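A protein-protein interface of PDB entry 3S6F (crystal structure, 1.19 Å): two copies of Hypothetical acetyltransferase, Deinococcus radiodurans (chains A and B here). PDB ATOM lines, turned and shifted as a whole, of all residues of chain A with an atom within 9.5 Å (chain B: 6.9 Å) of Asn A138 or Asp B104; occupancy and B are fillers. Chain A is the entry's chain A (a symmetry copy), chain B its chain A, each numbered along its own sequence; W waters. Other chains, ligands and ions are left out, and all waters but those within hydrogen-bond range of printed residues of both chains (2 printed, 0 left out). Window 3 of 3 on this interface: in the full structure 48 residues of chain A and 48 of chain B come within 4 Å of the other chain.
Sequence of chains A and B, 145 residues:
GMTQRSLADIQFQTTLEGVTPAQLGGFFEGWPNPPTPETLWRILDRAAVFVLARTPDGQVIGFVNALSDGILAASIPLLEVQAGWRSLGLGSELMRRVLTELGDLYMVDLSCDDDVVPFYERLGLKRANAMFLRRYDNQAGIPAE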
ATOM      1  N   PHE A  28     -14.306  11.900  15.579  1.00  0.00           N
ATOM      2  CA  PHE A  28     -13.111  12.749  15.466  1.00  0.00           C
ATOM      3  C   PHE A  28     -12.296  12.368  14.246  1.00  0.00           C
ATOM      4  O   PHE A  28     -11.056  12.412  14.254  1.00  0.00           O
ATOM      5  CB  PHE A  28     -12.293  12.752  16.747  1.00  0.00           C
ATOM      6  CG  PHE A  28     -13.123  13.116  17.953  1.00  0.00           C
ATOM      7  CD1 PHE A  28     -13.472  14.449  18.204  1.00  0.00           C
ATOM      8  CD2 PHE A  28     -13.515  12.135  18.849  1.00  0.00           C
ATOM      9  CE1 PHE A  28     -14.215  14.790  19.291  1.00  0.00           C
ATOM     10  CE2 PHE A  28     -14.240  12.488  19.952  1.00  0.00           C
ATOM     11  CZ  PHE A  28     -14.594  13.816  20.159  1.00  0.00           C
ATOM     12  N   TRP A  31      -8.892  14.236  13.198  1.00  0.00           N
ATOM     13  CA  TRP A  31      -8.250  14.898  14.323  1.00  0.00           C
ATOM     14  C   TRP A  31      -6.904  14.247  14.587  1.00  0.00           C
ATOM     15  O   TRP A  31      -6.835  13.041  14.741  1.00  0.00           O
ATOM     16  CB  TRP A  31      -9.086  14.799  15.584  1.00  0.00           C
ATOM     17  CG  TRP A  31     -10.330  15.663  15.587  1.00  0.00           C
ATOM     18  CD1 TRP A  31     -11.243  15.860  14.572  1.00  0.00           C
ATOM     19  CD2 TRP A  31     -10.802  16.411  16.701  1.00  0.00           C
ATOM     20  NE1 TRP A  31     -12.236  16.702  15.003  1.00  0.00           N
ATOM     21  CE2 TRP A  31     -11.981  17.070  16.295  1.00  0.00           C
ATOM     22  CE3 TRP A  31     -10.355  16.595  18.008  1.00  0.00           C
ATOM     23  CZ2 TRP A  31     -12.693  17.899  17.142  1.00  0.00           C
ATOM     24  CZ3 TRP A  31     -11.068  17.432  18.841  1.00  0.00           C
ATOM     25  CH2 TRP A  31     -12.214  18.078  18.402  1.00  0.00           C
ATOM     26  N   ASN A  33      -5.088  14.239  17.406  1.00  0.00           N
ATOM     27  CA  ASN A  33      -4.972  13.694  18.750  1.00  0.00           C
ATOM     28  C   ASN A  33      -6.333  13.759  19.407  1.00  0.00           C
ATOM     29  O   ASN A  33      -6.574  14.579  20.277  1.00  0.00           O
ATOM     30  CB  ASN A  33      -3.911  14.431  19.554  1.00  0.00           C
ATOM     31  CG  ASN A  33      -3.697  13.795  20.937  1.00  0.00           C
ATOM     32  OD1 ASN A  33      -3.863  12.604  21.092  1.00  0.00           O
ATOM     33  ND2 ASN A  33      -3.332  14.599  21.935  1.00  0.00           N
ATOM     34  N   PRO A  34      -7.246  12.881  18.990  1.00  0.00           N
ATOM     35  CA  PRO A  34      -8.619  12.930  19.363  1.00  0.00           C
ATOM     36  C   PRO A  34      -8.914  12.501  20.806  1.00  0.00           C
ATOM     37  O   PRO A  34      -8.246  11.629  21.330  1.00  0.00           O
ATOM     38  CB  PRO A  34      -9.220  11.915  18.355  1.00  0.00           C
ATOM     39  CG  PRO A  34      -8.206  10.922  18.170  1.00  0.00           C
ATOM     40  CD  PRO A  34      -7.007  11.767  18.056  1.00  0.00           C
ATOM     41  N   PRO A  35      -9.990  13.038  21.416  1.00  0.00           N
ATOM     42  CA  PRO A  35     -10.521  12.380  22.608  1.00  0.00           C
ATOM     43  C   PRO A  35     -10.802  10.920  22.333  1.00  0.00           C
ATOM     44  O   PRO A  35     -11.262  10.543  21.262  1.00  0.00           O
ATOM     45  CB  PRO A  35     -11.853  13.120  22.857  1.00  0.00           C
ATOM     46  CG  PRO A  35     -11.609  14.477  22.257  1.00  0.00           C
ATOM     47  CD  PRO A  35     -10.829  14.177  21.013  1.00  0.00           C
ATOM     48  N   THR A  36     -10.499  10.093  23.315  1.00  0.00           N
ATOM     49  CA  THR A  36     -10.887   8.690  23.287  1.00  0.00           C
ATOM     50  C   THR A  36     -12.409   8.552  23.401  1.00  0.00           C
ATOM     51  O   THR A  36     -13.096   9.481  23.820  1.00  0.00           O
ATOM     52  CB  THR A  36     -10.283   7.941  24.459  1.00  0.00           C
ATOM     53  OG1 THR A  36     -10.784   8.526  25.655  1.00  0.00           O
ATOM     54  CG2 THR A  36      -8.743   7.969  24.422  1.00  0.00           C
ATOM     55  N   THR A  39     -13.373   9.522  26.851  1.00  0.00           N
ATOM     56  CA  THR A  39     -13.432  10.954  27.004  1.00  0.00           C
ATOM     57  C   THR A  39     -14.673  11.546  26.363  1.00  0.00           C
ATOM     58  O   THR A  39     -15.292  12.457  26.914  1.00  0.00           O
ATOM     59  CB  THR A  39     -12.136  11.626  26.534  1.00  0.00           C
ATOM     60  OG1 THR A  39     -11.081  11.109  27.362  1.00  0.00           O
ATOM     61  CG2 THR A  39     -12.213  13.149  26.662  1.00  0.00           C
ATOM     62  N   ARG A  42     -17.496  11.293  28.686  1.00  0.00           N
ATOM     63  CA  ARG A  42     -17.440  12.359  29.704  1.00  0.00           C
ATOM     64  C   ARG A  42     -17.841  13.731  29.144  1.00  0.00           C
ATOM     65  O   ARG A  42     -18.540  14.501  29.819  1.00  0.00           O
ATOM     66  CB  ARG A  42     -16.083  12.416  30.380  1.00  0.00           C
ATOM     67  CG  ARG A  42     -15.689  11.165  31.148  1.00  0.00           C
ATOM     68  CD  ARG A  42     -14.340  11.373  31.937  1.00  0.00           C
ATOM     69  NE  ARG A  42     -13.151  11.641  31.064  1.00  0.00           N
ATOM     70  CZ  ARG A  42     -12.418  12.758  30.976  1.00  0.00           C
ATOM     71  NH1 ARG A  42     -12.686  13.847  31.696  1.00  0.00           N
ATOM     72  NH2 ARG A  42     -11.398  12.800  30.107  1.00  0.00           N
ATOM     73  N   ILE A  43     -17.405  14.023  27.913  1.00  0.00           N
ATOM     74  CA  ILE A  43     -17.817  15.271  27.262  1.00  0.00           C
ATOM     75  C   ILE A  43     -19.336  15.374  27.165  1.00  0.00           C
ATOM     76  O   ILE A  43     -19.929  16.391  27.504  1.00  0.00           O
ATOM     77  CB  ILE A  43     -17.123  15.398  25.859  1.00  0.00           C
ATOM     78  CG1 ILE A  43     -15.629  15.653  26.023  1.00  0.00           C
ATOM     79  CG2 ILE A  43     -17.783  16.481  25.028  1.00  0.00           C
ATOM     80  CD1 ILE A  43     -14.815  15.462  24.747  1.00  0.00           C
ATOM     81  N   LEU A 133      -9.686  30.373  20.133  1.00  0.00           N
ATOM     82  CA  LEU A 133      -8.411  29.822  20.582  1.00  0.00           C
ATOM     83  C   LEU A 133      -8.464  28.302  20.420  1.00  0.00           C
ATOM     84  O   LEU A 133      -9.498  27.680  20.717  1.00  0.00           O
ATOM     85  CB  LEU A 133      -8.120  30.128  22.068  1.00  0.00           C
ATOM     86  CG  LEU A 133      -7.994  31.589  22.375  1.00  0.00           C
ATOM     87  CD1 LEU A 133      -8.006  31.770  23.898  1.00  0.00           C
ATOM     88  CD2 LEU A 133      -6.752  32.195  21.743  1.00  0.00           C
ATOM     89  N   ARG A 134      -7.328  27.699  20.045  1.00  0.00           N
ATOM     90  CA  ARG A 134      -7.156  26.261  20.018  1.00  0.00           C
ATOM     91  C   ARG A 134      -5.913  25.896  20.782  1.00  0.00           C
ATOM     92  O   ARG A 134      -4.813  26.290  20.391  1.00  0.00           O
ATOM     93  CB  ARG A 134      -7.108  25.688  18.589  1.00  0.00           C
ATOM     94  CG  ARG A 134      -8.363  25.857  17.796  1.00  0.00           C
ATOM     95  CD  ARG A 134      -9.551  25.022  18.294  1.00  0.00           C
ATOM     96  NE  ARG A 134     -10.831  25.265  17.623  1.00  0.00           N
ATOM     97  CZ  ARG A 134     -11.819  26.025  18.072  1.00  0.00           C
ATOM     98  NH1 ARG A 134     -11.684  26.760  19.139  1.00  0.00           N
ATOM     99  NH2 ARG A 134     -12.951  26.112  17.388  1.00  0.00           N
ATOM    100  N   ARG A 135      -6.059  25.161  21.856  1.00  0.00           N
ATOM    101  CA  ARG A 135      -4.969  24.702  22.668  1.00  0.00           C
ATOM    102  C   ARG A 135      -4.679  23.265  22.303  1.00  0.00           C
ATOM    103  O   ARG A 135      -5.212  22.310  22.893  1.00  0.00           O
ATOM    104  CB  ARG A 135      -5.307  24.784  24.145  1.00  0.00           C
ATOM    105  CG  ARG A 135      -5.343  26.213  24.743  1.00  0.00           C
ATOM    106  CD  ARG A 135      -6.423  27.120  24.181  1.00  0.00           C
ATOM    107  NE  ARG A 135      -6.508  28.327  24.996  1.00  0.00           N
ATOM    108  CZ  ARG A 135      -7.169  28.449  26.131  1.00  0.00           C
ATOM    109  NH1 ARG A 135      -7.919  27.465  26.595  1.00  0.00           N
ATOM    110  NH2 ARG A 135      -7.052  29.559  26.842  1.00  0.00           N
ATOM    111  N   TYR A 136      -3.893  23.107  21.249  1.00  0.00           N
ATOM    112  CA  TYR A 136      -3.729  21.829  20.610  1.00  0.00           C
ATOM    113  C   TYR A 136      -3.106  20.786  21.536  1.00  0.00           C
ATOM    114  O   TYR A 136      -3.353  19.595  21.345  1.00  0.00           O
ATOM    115  CB  TYR A 136      -2.897  21.978  19.319  1.00  0.00           C
ATOM    116  CG  TYR A 136      -3.629  22.691  18.223  1.00  0.00           C
ATOM    117  CD1 TYR A 136      -4.628  22.062  17.489  1.00  0.00           C
ATOM    118  CD2 TYR A 136      -3.331  24.019  17.914  1.00  0.00           C
ATOM    119  CE1 TYR A 136      -5.320  22.768  16.471  1.00  0.00           C
ATOM    120  CE2 TYR A 136      -4.009  24.698  16.922  1.00  0.00           C
ATOM    121  CZ  TYR A 136      -4.973  24.072  16.203  1.00  0.00           C
ATOM    122  OH  TYR A 136      -5.670  24.745  15.215  1.00  0.00           O
ATOM    123  N   ASP A 137      -2.335  21.205  22.549  1.00  0.00           N
ATOM    124  CA  ASP A 137      -1.780  20.235  23.506  1.00  0.00           C
ATOM    125  C   ASP A 137      -2.875  19.446  24.208  1.00  0.00           C
ATOM    126  O   ASP A 137      -2.631  18.316  24.635  1.00  0.00           O
ATOM    127  CB  ASP A 137      -0.937  20.895  24.606  1.00  0.00           C
ATOM    128  CG  ASP A 137       0.312  21.594  24.143  1.00  0.00           C
ATOM    129  OD1 ASP A 137       0.701  21.447  22.977  1.00  0.00           O
ATOM    130  OD2 ASP A 137       0.907  22.269  25.020  1.00  0.00           O
ATOM    131  N   ASN A 138      -4.067  20.038  24.319  1.00  0.00           N
ATOM    132  CA  ASN A 138      -5.190  19.417  25.028  1.00  0.00           C
ATOM    133  C   ASN A 138      -6.327  19.006  24.140  1.00  0.00           C
ATOM    134  O   ASN A 138      -7.479  18.826  24.578  1.00  0.00           O
ATOM    135  CB  ASN A 138      -5.646  20.355  26.120  1.00  0.00           C
ATOM    136  CG  ASN A 138      -4.550  20.544  27.149  1.00  0.00           C
ATOM    137  OD1 ASN A 138      -3.790  19.598  27.453  1.00  0.00           O
ATOM    138  ND2 ASN A 138      -4.407  21.725  27.611  1.00  0.00           N
ATOM    139  N   GLN A 139      -6.014  18.721  22.877  1.00  0.00           N
ATOM    140  CA  GLN A 139      -6.989  18.253  21.929  1.00  0.00           C
ATOM    141  C   GLN A 139      -7.719  16.963  22.334  1.00  0.00           C
ATOM    142  O   GLN A 139      -8.855  16.755  21.910  1.00  0.00           O
ATOM    143  CB  GLN A 139      -6.336  18.145  20.548  1.00  0.00           C
ATOM    144  CG  GLN A 139      -7.320  17.865  19.405  1.00  0.00           C
ATOM    145  CD  GLN A 139      -6.568  17.853  18.077  1.00  0.00           C
ATOM    146  OE1 GLN A 139      -6.064  16.847  17.658  1.00  0.00           O
ATOM    147  NE2 GLN A 139      -6.426  19.041  17.425  1.00  0.00           N
ATOM    148  N   ALA A 140      -7.074  16.106  23.127  1.00  0.00           N
ATOM    149  CA  ALA A 140      -7.692  14.866  23.558  1.00  0.00           C
ATOM    150  C   ALA A 140      -8.531  15.017  24.822  1.00  0.00           C
ATOM    151  O   ALA A 140      -9.112  14.036  25.307  1.00  0.00           O
ATOM    152  CB  ALA A 140      -6.628  13.753  23.719  1.00  0.00           C
ATOM    153  N   GLY A 141      -8.634  16.238  25.338  1.00  0.00           N
ATOM    154  CA  GLY A 141      -9.473  16.544  26.498  1.00  0.00           C
ATOM    155  C   GLY A 141      -8.704  16.643  27.776  1.00  0.00           C
ATOM    156  O   GLY A 141      -7.695  15.971  27.956  1.00  0.00           O
ATOM    157  N   ILE A 142      -9.208  17.417  28.711  1.00  0.00           N
ATOM    158  CA  ILE A 142      -8.640  17.444  30.068  1.00  0.00           C
ATOM    159  C   ILE A 142      -8.978  16.148  30.792  1.00  0.00           C
ATOM    160  O   ILE A 142     -10.152  15.728  30.852  1.00  0.00           O
ATOM    161  CB  ILE A 142      -9.260  18.606  30.903  1.00  0.00           C
ATOM    162  CG1 ILE A 142      -9.037  19.936  30.219  1.00  0.00           C
ATOM    163  CG2 ILE A 142      -8.719  18.587  32.318  1.00  0.00           C
ATOM    164  CD1 ILE A 142      -7.590  20.209  29.763  1.00  0.00           C
ATOM    165  N   PRO A 143      -7.970  15.472  31.366  1.00  0.00           N
ATOM    166  CA  PRO A 143      -8.266  14.173  32.014  1.00  0.00           C
ATOM    167  C   PRO A 143      -9.169  14.288  33.220  1.00  0.00           C
ATOM    168  O   PRO A 143      -9.220  15.353  33.878  1.00  0.00           O
ATOM    169  CB  PRO A 143      -6.890  13.672  32.477  1.00  0.00           C
ATOM    170  CG  PRO A 143      -5.910  14.399  31.640  1.00  0.00           C
ATOM    171  CD  PRO A 143      -6.527  15.725  31.246  1.00  0.00           C
ATOM    172  N   ILE B  71     -13.883  20.103  29.833  1.00  0.00           N
ATOM    173  CA  ILE B  71     -13.083  19.017  29.265  1.00  0.00           C
ATOM    174  C   ILE B  71     -12.508  19.368  27.913  1.00  0.00           C
ATOM    175  O   ILE B  71     -11.329  19.060  27.649  1.00  0.00           O
ATOM    176  CB  ILE B  71     -13.875  17.698  29.148  1.00  0.00           C
ATOM    177  CG1 ILE B  71     -14.383  17.230  30.504  1.00  0.00           C
ATOM    178  CG2 ILE B  71     -13.062  16.589  28.460  1.00  0.00           C
ATOM    179  CD1 ILE B  71     -15.426  16.099  30.449  1.00  0.00           C
ATOM    180  N   LEU B  72     -13.311  19.970  27.038  1.00  0.00           N
ATOM    181  CA  LEU B  72     -12.886  20.246  25.662  1.00  0.00           C
ATOM    182  C   LEU B  72     -13.235  21.640  25.182  1.00  0.00           C
ATOM    183  O   LEU B  72     -12.502  22.169  24.339  1.00  0.00           O
ATOM    184  CB  LEU B  72     -13.454  19.212  24.703  1.00  0.00           C
ATOM    185  CG  LEU B  72     -12.716  19.080  23.359  1.00  0.00           C
ATOM    186  CD1 LEU B  72     -11.383  18.379  23.543  1.00  0.00           C
ATOM    187  CD2 LEU B  72     -13.611  18.380  22.308  1.00  0.00           C
ATOM    188  N   LEU B  99     -10.275  33.592  30.759  1.00  0.00           N
ATOM    189  CA  LEU B  99      -9.513  32.506  30.160  1.00  0.00           C
ATOM    190  C   LEU B  99      -8.754  31.735  31.247  1.00  0.00           C
ATOM    191  O   LEU B  99      -8.705  30.505  31.208  1.00  0.00           O
ATOM    192  CB  LEU B  99      -8.591  33.025  29.043  1.00  0.00           C
ATOM    193  CG  LEU B  99      -9.310  33.560  27.811  1.00  0.00           C
ATOM    194  CD1 LEU B  99      -8.330  34.311  26.903  1.00  0.00           C
ATOM    195  CD2 LEU B  99     -10.034  32.464  27.065  1.00  0.00           C
ATOM    196  N   THR B 100      -8.245  32.428  32.248  1.00  0.00           N
ATOM    197  CA  THR B 100      -7.610  31.767  33.390  1.00  0.00           C
ATOM    198  C   THR B 100      -8.627  30.895  34.131  1.00  0.00           C
ATOM    199  O   THR B 100      -8.339  29.730  34.493  1.00  0.00           O
ATOM    200  CB  THR B 100      -6.967  32.774  34.318  1.00  0.00           C
ATOM    201  OG1 THR B 100      -5.906  33.431  33.597  1.00  0.00           O
ATOM    202  CG2 THR B 100      -6.449  32.117  35.606  1.00  0.00           C
ATOM    203  N   LEU B 102     -11.285  29.454  32.962  1.00  0.00           N
ATOM    204  CA  LEU B 102     -11.667  28.341  32.111  1.00  0.00           C
ATOM    205  C   LEU B 102     -10.633  27.239  32.069  1.00  0.00           C
ATOM    206  O   LEU B 102     -10.978  26.071  31.860  1.00  0.00           O
ATOM    207  CB  LEU B 102     -11.943  28.823  30.681  1.00  0.00           C
ATOM    208  CG  LEU B 102     -13.278  29.543  30.496  1.00  0.00           C
ATOM    209  CD1 LEU B 102     -13.318  30.246  29.163  1.00  0.00           C
ATOM    210  CD2 LEU B 102     -14.447  28.572  30.698  1.00  0.00           C
ATOM    211  N   GLY B 103      -9.366  27.592  32.213  1.00  0.00           N
ATOM    212  CA  GLY B 103      -8.276  26.656  32.049  1.00  0.00           C
ATOM    213  C   GLY B 103      -7.922  26.402  30.583  1.00  0.00           C
ATOM    214  O   GLY B 103      -8.451  26.998  29.653  1.00  0.00           O
ATOM    215  N   ASP B 104      -6.985  25.487  30.344  1.00  0.00           N
ATOM    216  CA  ASP B 104      -6.403  25.311  29.004  1.00  0.00           C
ATOM    217  C   ASP B 104      -7.161  24.337  28.102  1.00  0.00           C
ATOM    218  O   ASP B 104      -6.580  23.574  27.366  1.00  0.00           O
ATOM    219  CB  ASP B 104      -4.925  24.935  29.109  1.00  0.00           C
ATOM    220  CG  ASP B 104      -4.046  26.119  29.516  1.00  0.00           C
ATOM    221  OD1 ASP B 104      -4.462  27.295  29.355  1.00  0.00           O
ATOM    222  OD2 ASP B 104      -2.920  25.841  29.945  1.00  0.00           O
ATOM    223  N   LEU B 105      -8.475  24.390  28.153  1.00  0.00           N
ATOM    224  CA  LEU B 105      -9.406  23.691  27.241  1.00  0.00           C
ATOM    225  C   LEU B 105      -8.990  23.788  25.824  1.00  0.00           C
ATOM    226  O   LEU B 105      -8.543  24.863  25.384  1.00  0.00           O
ATOM    227  CB  LEU B 105     -10.779  24.369  27.258  1.00  0.00           C
ATOM    228  CG  LEU B 105     -11.490  24.366  28.588  1.00  0.00           C
ATOM    229  CD1 LEU B 105     -12.752  25.226  28.559  1.00  0.00           C
ATOM    230  CD2 LEU B 105     -11.748  22.892  29.061  1.00  0.00           C
ATOM    231  N   TYR B 106      -9.228  22.766  25.038  1.00  0.00           N
ATOM    232  CA  TYR B 106      -8.917  22.783  23.646  1.00  0.00           C
ATOM    233  C   TYR B 106      -9.552  23.935  22.873  1.00  0.00           C
ATOM    234  O   TYR B 106      -8.868  24.634  22.116  1.00  0.00           O
ATOM    235  CB  TYR B 106      -9.297  21.416  23.016  1.00  0.00           C
ATOM    236  CG  TYR B 106      -9.075  21.373  21.519  1.00  0.00           C
ATOM    237  CD1 TYR B 106      -7.847  21.754  20.994  1.00  0.00           C
ATOM    238  CD2 TYR B 106     -10.061  20.984  20.646  1.00  0.00           C
ATOM    239  CE1 TYR B 106      -7.642  21.783  19.653  1.00  0.00           C
ATOM    240  CE2 TYR B 106      -9.851  20.982  19.261  1.00  0.00           C
ATOM    241  CZ  TYR B 106      -8.606  21.414  18.780  1.00  0.00           C
ATOM    242  OH  TYR B 106      -8.332  21.511  17.435  1.00  0.00           O
ATOM    243  N   MET B 107     -10.851  24.147  23.072  1.00  0.00           N
ATOM    244  CA  MET B 107     -11.596  25.146  22.301  1.00  0.00           C
ATOM    245  C   MET B 107     -12.159  26.233  23.190  1.00  0.00           C
ATOM    246  O   MET B 107     -12.861  25.936  24.147  1.00  0.00           O
ATOM    247  CB  MET B 107     -12.790  24.497  21.597  1.00  0.00           C
ATOM    248  CG  MET B 107     -12.420  23.431  20.617  1.00  0.00           C
ATOM    249  SD  MET B 107     -13.949  22.260  20.192  1.00  0.00           S
ATOM    250  CE  MET B 107     -15.155  23.570  19.498  1.00  0.00           C
ATOM    251  N   VAL B 108     -11.914  27.485  22.817  1.00  0.00           N
ATOM    252  CA  VAL B 108     -12.634  28.631  23.375  1.00  0.00           C
ATOM    253  C   VAL B 108     -13.082  29.454  22.190  1.00  0.00           C
ATOM    254  O   VAL B 108     -12.247  29.815  21.334  1.00  0.00           O
ATOM    255  CB  VAL B 108     -11.793  29.495  24.305  1.00  0.00           C
ATOM    256  CG1 VAL B 108     -12.658  30.609  24.903  1.00  0.00           C
ATOM    257  CG2 VAL B 108     -11.177  28.624  25.454  1.00  0.00           C
HETATM  258  O   HOH W   1      -8.984  29.344  28.727  1.00  0.00           O
HETATM  259  O   HOH W   2      -9.193  20.211  26.325  1.00  0.00           O
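No position is printed for both chains. Of the 25 pairs that touch across the chains among the printed residues, none has its exchanged pair printed and touching as well.
Water W1 lies within hydrogen-bond range of O of Gly B103 (2.6 Å), NH2 of Arg A135 (2.7 Å) and O of Leu B99 (2.8 Å). Water W2 lies within hydrogen-bond range of the backbone carbonyl oxygen of Ile B71 (2.8 Å), the backbone carbonyl oxygen of Asn A138 (2.8 Å) and the backbone NH of Tyr B106 (2.9 Å).
Of the printed residues of chain B, Asn A138 touches Asp B104 (2.9 Å) and Tyr B106 (3.5 Å). Printed residues of chain A within 4 Å of Asp B104: Arg A135 (3.6 Å) and Asn A138 (2.9 Å). Printed residues of chain A within 4 Å of Gly B103: Arg A135. Printed residues of chain B within 4 Å of Arg A135: Gly B103 (3.1 Å), Asp B104 (3.6 Å), Leu B105 (2.9 Å), Tyr B106 (2.9 Å) and Val B108 (3.6 Å). Of the printed residues of chain B, Thr A39 touches Ile B71. Asp A137 touches none of the printed residues of chain B. Thr B100 touches none of the printed residues of chain A.
The backbone carbonyl oxygen (O) of Leu B72 lies within hydrogen-bond range of the backbone NH (N) of Tyr B106 (3.4 Å). O of Leu B72 is in hydrogen-bond range of N of Met B107, 2.9 Å away. N of Asn A33 sits at hydrogen-bond distance from OE1 of Gln A139 (2.8 Å). The side-chain hydroxyl (OG1) of Thr A36 is in hydrogen-bond range of the backbone NH (N) of Thr A39, 3.0 Å away. The side-chain hydroxyl of Thr A39 sits at hydrogen-bond distance from the guanidinium group of Arg A42 (3.2 Å). NH1 of Arg A42 is in hydrogen-bond range of O of Ile A142.
N of Ile A142 sits at hydrogen-bond distance from O of Ile B71. The backbone carbonyl oxygen (O) of Gly B103 lies within hydrogen-bond range of the guanidinium group (NH1) of Arg A135, 3.1 Å away. The backbone carbonyl oxygen of Asp B104 is in hydrogen-bond range of the side-chain amide nitrogen of Asn A138, 2.9 Å away. The backbone carbonyl oxygen (O) of Leu B105 sits at hydrogen-bond distance from the guanidinium group (NH1) of Arg A135, 2.9 Å away. The backbone NH (N) of Arg A135 sits at hydrogen-bond distance from the backbone carbonyl oxygen (O) of Tyr B106, 2.9 Å away. OH of Tyr B106 lies within hydrogen-bond range of NE2 of Gln A139, 3.1 Å away. O of Val B108 lies within hydrogen-bond range of N of Leu A133 (2.9 Å). O of Tyr B106 lies close to O of Leu A133, 3.4 Å away.
CG2 of Thr A39 touches CG2 of Ile B71, 3.97 Å away. Ile A43 touches Ile B71 (CG1 to CG2, 3.7 Å). Leu A133 touches Met B107 (O to CA, 3.7 Å). Arg A134 touches Met B107. NH1 of Arg A134 touches N of Val B108, at 3.8 Å. Arg A135 touches Val B108. OH of Tyr B106 touches CE1 of Tyr A136, 3.4 Å away. CD1 of Leu B72 touches O of Gln A139, 3.4 Å away. Gly A141 touches Ile B71. Leu B72 touches Gly A141 (CD1 to N, 3.9 Å).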
